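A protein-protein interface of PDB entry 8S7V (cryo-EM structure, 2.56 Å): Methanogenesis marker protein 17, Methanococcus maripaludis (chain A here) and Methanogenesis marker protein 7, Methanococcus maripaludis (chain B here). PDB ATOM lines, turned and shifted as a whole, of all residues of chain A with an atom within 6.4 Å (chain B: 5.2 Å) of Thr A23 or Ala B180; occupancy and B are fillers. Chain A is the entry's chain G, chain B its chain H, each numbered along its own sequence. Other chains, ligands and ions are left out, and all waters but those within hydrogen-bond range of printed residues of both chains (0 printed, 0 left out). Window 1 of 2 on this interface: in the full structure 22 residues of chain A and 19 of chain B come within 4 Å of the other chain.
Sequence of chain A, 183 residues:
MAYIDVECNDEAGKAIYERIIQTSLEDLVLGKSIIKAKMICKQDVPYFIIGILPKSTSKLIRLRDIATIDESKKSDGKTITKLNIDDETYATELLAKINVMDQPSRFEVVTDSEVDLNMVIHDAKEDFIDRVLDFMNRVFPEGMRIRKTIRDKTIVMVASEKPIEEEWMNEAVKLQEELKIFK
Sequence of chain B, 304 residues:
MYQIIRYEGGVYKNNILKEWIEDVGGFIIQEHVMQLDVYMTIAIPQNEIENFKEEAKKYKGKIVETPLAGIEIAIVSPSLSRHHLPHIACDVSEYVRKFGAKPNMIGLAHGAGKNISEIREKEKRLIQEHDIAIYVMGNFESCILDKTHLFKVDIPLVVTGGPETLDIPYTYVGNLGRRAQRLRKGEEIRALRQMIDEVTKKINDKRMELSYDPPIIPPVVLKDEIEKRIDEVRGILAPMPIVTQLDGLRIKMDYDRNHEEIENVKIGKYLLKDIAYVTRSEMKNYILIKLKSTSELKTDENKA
The side-chain amide oxygen of Gln B181 lies within hydrogen-bond range of the guanidinium group of Arg A19 (3.2 Å). The side-chain hydroxyl (OG1) of Thr A23 sits at hydrogen-bond distance from the side-chain amide oxygen (OE1) of Gln B181 (2.6 Å). The backbone carbonyl oxygen (O) of Arg A138 lies within hydrogen-bond range of the guanidinium group (NH2) of Arg B178 (2.8 Å).
OG1 of Thr A23 lies close to O of Arg A19 (3.4 Å). The backbone carbonyl oxygen (O) of Ile A20 is in hydrogen-bond range of the side-chain hydroxyl (OG) of Ser A24, at 3.1 Å. The side-chain carboxylate (OD2) of Asp A27 lies within salt-bridge range of the guanidinium group (NH1) of Arg A138, at 3.9 Å.
O of Arg B178 touches CD1 of Ile A20, at 3.2 Å. Thr A23 touches Ala B180 (CG2 to CB, 3.6 Å).
Of chain B, only Ala B180 (3.6 Å) and Gln B181 (2.6 Å) come within 4 Å of Thr A23. Of the printed residues of chain B, Arg A19 touches Gln B181 (3.2 Å). Of the printed residues of chain B, Ile A20 touches Arg B178 (3.2 Å). The nearest printed residue of chain B that does not touch Thr A23 is Arg B179 (6.7 Å).
Printed residues of chain B that touch a printed residue of chain A: Arg B178, Ala B180 and Gln B181. Hydrophobic or aromatic side chains of chain B within 4 Å of the printed part of chain A: Ala B180. Hydrophobic or aromatic side chains of chain A within 4 Å of the printed part of chain B: Ile A20. Along chain A the printed residues that touch a printed residue of chain B span positions 19 to 138. Among the printed residues, no Asp or Glu carboxylate lies within 4 Å of a Lys or Arg side-chain nitrogen of the other chain.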
ATOM      1  N   ILE A   4     -15.741  31.718  10.915  1.00  0.00           N
ATOM      2  CA  ILE A   4     -17.060  31.214  10.555  1.00  0.00           C
ATOM      3  C   ILE A   4     -17.523  30.257  11.640  1.00  0.00           C
ATOM      4  O   ILE A   4     -16.831  29.280  11.951  1.00  0.00           O
ATOM      5  CB  ILE A   4     -17.044  30.512   9.184  1.00  0.00           C
ATOM      6  CG1 ILE A   4     -16.564  31.472   8.097  1.00  0.00           C
ATOM      7  CG2 ILE A   4     -18.421  29.972   8.850  1.00  0.00           C
ATOM      8  CD1 ILE A   4     -16.310  30.803   6.772  1.00  0.00           C
ATOM      9  N   GLU A  18     -21.930  25.999   7.099  1.00  0.00           N
ATOM     10  CA  GLU A  18     -20.581  26.533   7.251  1.00  0.00           C
ATOM     11  C   GLU A  18     -19.850  26.530   5.917  1.00  0.00           C
ATOM     12  O   GLU A  18     -19.202  27.519   5.550  1.00  0.00           O
ATOM     13  CB  GLU A  18     -19.809  25.722   8.289  1.00  0.00           C
ATOM     14  CG  GLU A  18     -19.675  26.401   9.639  1.00  0.00           C
ATOM     15  CD  GLU A  18     -19.597  25.412  10.785  1.00  0.00           C
ATOM     16  OE1 GLU A  18     -19.744  25.835  11.950  1.00  0.00           O
ATOM     17  OE2 GLU A  18     -19.389  24.209  10.520  1.00  0.00           O
ATOM     18  N   ARG A  19     -19.962  25.430   5.170  1.00  0.00           N
ATOM     19  CA  ARG A  19     -19.374  25.388   3.835  1.00  0.00           C
ATOM     20  C   ARG A  19     -20.017  26.412   2.907  1.00  0.00           C
ATOM     21  O   ARG A  19     -19.328  27.023   2.085  1.00  0.00           O
ATOM     22  CB  ARG A  19     -19.502  23.984   3.248  1.00  0.00           C
ATOM     23  CG  ARG A  19     -18.408  23.032   3.691  1.00  0.00           C
ATOM     24  CD  ARG A  19     -17.564  22.587   2.511  1.00  0.00           C
ATOM     25  NE  ARG A  19     -17.183  23.713   1.666  1.00  0.00           N
ATOM     26  CZ  ARG A  19     -15.997  24.301   1.694  1.00  0.00           C
ATOM     27  NH1 ARG A  19     -15.043  23.895   2.515  1.00  0.00           N
ATOM     28  NH2 ARG A  19     -15.760  25.324   0.877  1.00  0.00           N
ATOM     29  N   ILE A  20     -21.333  26.606   3.020  1.00  0.00           N
ATOM     30  CA  ILE A  20     -22.023  27.592   2.191  1.00  0.00           C
ATOM     31  C   ILE A  20     -21.514  28.997   2.490  1.00  0.00           C
ATOM     32  O   ILE A  20     -21.275  29.794   1.575  1.00  0.00           O
ATOM     33  CB  ILE A  20     -23.546  27.491   2.396  1.00  0.00           C
ATOM     34  CG1 ILE A  20     -24.089  26.212   1.765  1.00  0.00           C
ATOM     35  CG2 ILE A  20     -24.245  28.699   1.806  1.00  0.00           C
ATOM     36  CD1 ILE A  20     -25.511  25.911   2.158  1.00  0.00           C
ATOM     37  N   ILE A  21     -21.354  29.327   3.773  1.00  0.00           N
ATOM     38  CA  ILE A  21     -20.840  30.641   4.153  1.00  0.00           C
ATOM     39  C   ILE A  21     -19.422  30.829   3.633  1.00  0.00           C
ATOM     40  O   ILE A  21     -19.079  31.887   3.088  1.00  0.00           O
ATOM     41  CB  ILE A  21     -20.909  30.821   5.681  1.00  0.00           C
ATOM     42  CG1 ILE A  21     -22.359  30.865   6.154  1.00  0.00           C
ATOM     43  CG2 ILE A  21     -20.183  32.085   6.104  1.00  0.00           C
ATOM     44  CD1 ILE A  21     -22.515  30.692   7.644  1.00  0.00           C
ATOM     45  N   GLN A  22     -18.578  29.807   3.790  1.00  0.00           N
ATOM     46  CA  GLN A  22     -17.212  29.905   3.287  1.00  0.00           C
ATOM     47  C   GLN A  22     -17.192  30.126   1.779  1.00  0.00           C
ATOM     48  O   GLN A  22     -16.444  30.971   1.276  1.00  0.00           O
ATOM     49  CB  GLN A  22     -16.430  28.645   3.648  1.00  0.00           C
ATOM     50  CG  GLN A  22     -15.151  28.468   2.858  1.00  0.00           C
ATOM     51  CD  GLN A  22     -14.114  27.664   3.606  1.00  0.00           C
ATOM     52  OE1 GLN A  22     -14.423  26.995   4.591  1.00  0.00           O
ATOM     53  NE2 GLN A  22     -12.874  27.717   3.139  1.00  0.00           N
ATOM     54  N   THR A  23     -18.019  29.381   1.044  1.00  0.00           N
ATOM     55  CA  THR A  23     -18.042  29.507  -0.408  1.00  0.00           C
ATOM     56  C   THR A  23     -18.559  30.872  -0.839  1.00  0.00           C
ATOM     57  O   THR A  23     -18.025  31.476  -1.774  1.00  0.00           O
ATOM     58  CB  THR A  23     -18.889  28.387  -1.006  1.00  0.00           C
ATOM     59  OG1 THR A  23     -18.098  27.200  -1.088  1.00  0.00           O
ATOM     60  CG2 THR A  23     -19.368  28.755  -2.400  1.00  0.00           C
ATOM     61  N   SER A  24     -19.595  31.377  -0.167  1.00  0.00           N
ATOM     62  CA  SER A  24     -20.110  32.699  -0.497  1.00  0.00           C
ATOM     63  C   SER A  24     -19.090  33.789  -0.198  1.00  0.00           C
ATOM     64  O   SER A  24     -19.029  34.791  -0.917  1.00  0.00           O
ATOM     65  CB  SER A  24     -21.408  32.958   0.262  1.00  0.00           C
ATOM     66  OG  SER A  24     -22.431  32.082  -0.178  1.00  0.00           O
ATOM     67  N   LEU A  25     -18.292  33.619   0.858  1.00  0.00           N
ATOM     68  CA  LEU A  25     -17.219  34.572   1.121  1.00  0.00           C
ATOM     69  C   LEU A  25     -16.143  34.504   0.043  1.00  0.00           C
ATOM     70  O   LEU A  25     -15.646  35.541  -0.410  1.00  0.00           O
ATOM     71  CB  LEU A  25     -16.614  34.317   2.499  1.00  0.00           C
ATOM     72  CG  LEU A  25     -17.416  34.834   3.693  1.00  0.00           C
ATOM     73  CD1 LEU A  25     -16.782  34.386   4.997  1.00  0.00           C
ATOM     74  CD2 LEU A  25     -17.532  36.346   3.644  1.00  0.00           C
ATOM     75  N   GLU A  26     -15.765  33.293  -0.374  1.00  0.00           N
ATOM     76  CA  GLU A  26     -14.733  33.152  -1.401  1.00  0.00           C
ATOM     77  C   GLU A  26     -15.190  33.716  -2.743  1.00  0.00           C
ATOM     78  O   GLU A  26     -14.404  34.352  -3.453  1.00  0.00           O
ATOM     79  CB  GLU A  26     -14.333  31.686  -1.556  1.00  0.00           C
ATOM     80  CG  GLU A  26     -13.801  31.040  -0.296  1.00  0.00           C
ATOM     81  CD  GLU A  26     -12.991  29.795  -0.579  1.00  0.00           C
ATOM     82  OE1 GLU A  26     -12.300  29.758  -1.618  1.00  0.00           O
ATOM     83  OE2 GLU A  26     -13.047  28.849   0.234  1.00  0.00           O
ATOM     84  N   ASP A  27     -16.451  33.478  -3.112  1.00  0.00           N
ATOM     85  CA  ASP A  27     -16.936  33.890  -4.426  1.00  0.00           C
ATOM     86  C   ASP A  27     -16.917  35.404  -4.576  1.00  0.00           C
ATOM     87  O   ASP A  27     -16.535  35.925  -5.630  1.00  0.00           O
ATOM     88  CB  ASP A  27     -18.347  33.349  -4.656  1.00  0.00           C
ATOM     89  CG  ASP A  27     -18.345  31.961  -5.266  1.00  0.00           C
ATOM     90  OD1 ASP A  27     -17.260  31.482  -5.652  1.00  0.00           O
ATOM     91  OD2 ASP A  27     -19.431  31.350  -5.360  1.00  0.00           O
ATOM     92  N   LEU A  28     -17.324  36.126  -3.538  1.00  0.00           N
ATOM     93  CA  LEU A  28     -17.325  37.579  -3.553  1.00  0.00           C
ATOM     94  C   LEU A  28     -15.972  38.173  -3.195  1.00  0.00           C
ATOM     95  O   LEU A  28     -15.833  39.401  -3.195  1.00  0.00           O
ATOM     96  CB  LEU A  28     -18.392  38.109  -2.594  1.00  0.00           C
ATOM     97  CG  LEU A  28     -19.824  38.094  -3.125  1.00  0.00           C
ATOM     98  CD1 LEU A  28     -20.805  38.496  -2.039  1.00  0.00           C
ATOM     99  CD2 LEU A  28     -19.951  39.013  -4.328  1.00  0.00           C
ATOM    100  N   ARG A 138     -26.852  35.582  -0.923  1.00  0.00           N
ATOM    101  CA  ARG A 138     -26.360  34.272  -1.332  1.00  0.00           C
ATOM    102  C   ARG A 138     -26.551  33.231  -0.234  1.00  0.00           C
ATOM    103  O   ARG A 138     -26.995  32.111  -0.508  1.00  0.00           O
ATOM    104  CB  ARG A 138     -24.887  34.365  -1.723  1.00  0.00           C
ATOM    105  CG  ARG A 138     -24.650  34.772  -3.161  1.00  0.00           C
ATOM    106  CD  ARG A 138     -23.166  34.885  -3.455  1.00  0.00           C
ATOM    107  NE  ARG A 138     -22.877  35.956  -4.400  1.00  0.00           N
ATOM    108  CZ  ARG A 138     -22.106  35.822  -5.470  1.00  0.00           C
ATOM    109  NH1 ARG A 138     -21.525  34.671  -5.764  1.00  0.00           N
ATOM    110  NH2 ARG A 138     -21.910  36.871  -6.264  1.00  0.00           N
ATOM    111  N   HIS B  87     -25.962  24.492  -8.696  1.00  0.00           N
ATOM    112  CA  HIS B  87     -25.170  23.453  -8.054  1.00  0.00           C
ATOM    113  C   HIS B  87     -26.088  22.545  -7.250  1.00  0.00           C
ATOM    114  O   HIS B  87     -27.111  22.979  -6.719  1.00  0.00           O
ATOM    115  CB  HIS B  87     -24.066  24.040  -7.172  1.00  0.00           C
ATOM    116  CG  HIS B  87     -22.819  24.369  -7.927  1.00  0.00           C
ATOM    117  ND1 HIS B  87     -22.159  23.443  -8.704  1.00  0.00           N
ATOM    118  CD2 HIS B  87     -22.128  25.526  -8.051  1.00  0.00           C
ATOM    119  CE1 HIS B  87     -21.105  24.011  -9.262  1.00  0.00           C
ATOM    120  NE2 HIS B  87     -21.062  25.275  -8.882  1.00  0.00           N
ATOM    121  N   ARG B 178     -28.603  21.303   0.108  1.00  0.00           N
ATOM    122  CA  ARG B 178     -28.398  22.519  -0.664  1.00  0.00           C
ATOM    123  C   ARG B 178     -26.966  22.994  -0.456  1.00  0.00           C
ATOM    124  O   ARG B 178     -26.565  23.292   0.673  1.00  0.00           O
ATOM    125  CB  ARG B 178     -29.395  23.592  -0.241  1.00  0.00           C
ATOM    126  CG  ARG B 178     -29.149  24.943  -0.871  1.00  0.00           C
ATOM    127  CD  ARG B 178     -28.929  26.003   0.186  1.00  0.00           C
ATOM    128  NE  ARG B 178     -28.321  27.203  -0.373  1.00  0.00           N
ATOM    129  CZ  ARG B 178     -28.345  28.394   0.207  1.00  0.00           C
ATOM    130  NH1 ARG B 178     -28.936  28.581   1.375  1.00  0.00           N
ATOM    131  NH2 ARG B 178     -27.761  29.423  -0.400  1.00  0.00           N
ATOM    132  N   ARG B 179     -26.193  23.052  -1.536  1.00  0.00           N
ATOM    133  CA  ARG B 179     -24.801  23.468  -1.463  1.00  0.00           C
ATOM    134  C   ARG B 179     -24.556  24.566  -2.486  1.00  0.00           C
ATOM    135  O   ARG B 179     -25.467  25.006  -3.192  1.00  0.00           O
ATOM    136  CB  ARG B 179     -23.849  22.290  -1.697  1.00  0.00           C
ATOM    137  CG  ARG B 179     -23.517  21.505  -0.443  1.00  0.00           C
ATOM    138  CD  ARG B 179     -24.112  20.111  -0.496  1.00  0.00           C
ATOM    139  NE  ARG B 179     -23.796  19.333   0.695  1.00  0.00           N
ATOM    140  CZ  ARG B 179     -22.775  18.493   0.794  1.00  0.00           C
ATOM    141  NH1 ARG B 179     -21.936  18.304  -0.210  1.00  0.00           N
ATOM    142  NH2 ARG B 179     -22.591  17.827   1.930  1.00  0.00           N
ATOM    143  N   ALA B 180     -23.305  25.017  -2.553  1.00  0.00           N
ATOM    144  CA  ALA B 180     -22.906  26.059  -3.487  1.00  0.00           C
ATOM    145  C   ALA B 180     -21.646  25.716  -4.266  1.00  0.00           C
ATOM    146  O   ALA B 180     -21.181  26.544  -5.056  1.00  0.00           O
ATOM    147  CB  ALA B 180     -22.709  27.387  -2.747  1.00  0.00           C
ATOM    148  N   GLN B 181     -21.081  24.528  -4.073  1.00  0.00           N
ATOM    149  CA  GLN B 181     -19.902  24.087  -4.798  1.00  0.00           C
ATOM    150  C   GLN B 181     -20.246  22.897  -5.679  1.00  0.00           C
ATOM    151  O   GLN B 181     -21.267  22.231  -5.494  1.00  0.00           O
ATOM    152  CB  GLN B 181     -18.766  23.691  -3.849  1.00  0.00           C
ATOM    153  CG  GLN B 181     -18.337  24.773  -2.896  1.00  0.00           C
ATOM    154  CD  GLN B 181     -16.899  25.195  -3.112  1.00  0.00           C
ATOM    155  OE1 GLN B 181     -16.268  25.766  -2.223  1.00  0.00           O
ATOM    156  NE2 GLN B 181     -16.371  24.915  -4.296  1.00  0.00           N
ATOM    157  N   ARG B 182     -19.372  22.638  -6.645  1.00  0.00           N
ATOM    158  CA  ARG B 182     -19.493  21.438  -7.454  1.00  0.00           C
ATOM    159  C   ARG B 182     -19.236  20.207  -6.596  1.00  0.00           C
ATOM    160  O   ARG B 182     -18.302  20.178  -5.790  1.00  0.00           O
ATOM    161  CB  ARG B 182     -18.511  21.488  -8.622  1.00  0.00           C
ATOM    162  CG  ARG B 182     -18.451  20.218  -9.442  1.00  0.00           C
ATOM    163  CD  ARG B 182     -19.287  20.346 -10.700  1.00  0.00           C
ATOM    164  NE  ARG B 182     -18.933  19.340 -11.692  1.00  0.00           N
ATOM    165  CZ  ARG B 182     -19.527  18.160 -11.802  1.00  0.00           C
ATOM    166  NH1 ARG B 182     -20.506  17.802 -10.990  1.00  0.00           N
ATOM    167  NH2 ARG B 182     -19.127  17.318 -12.750  1.00  0.00           N
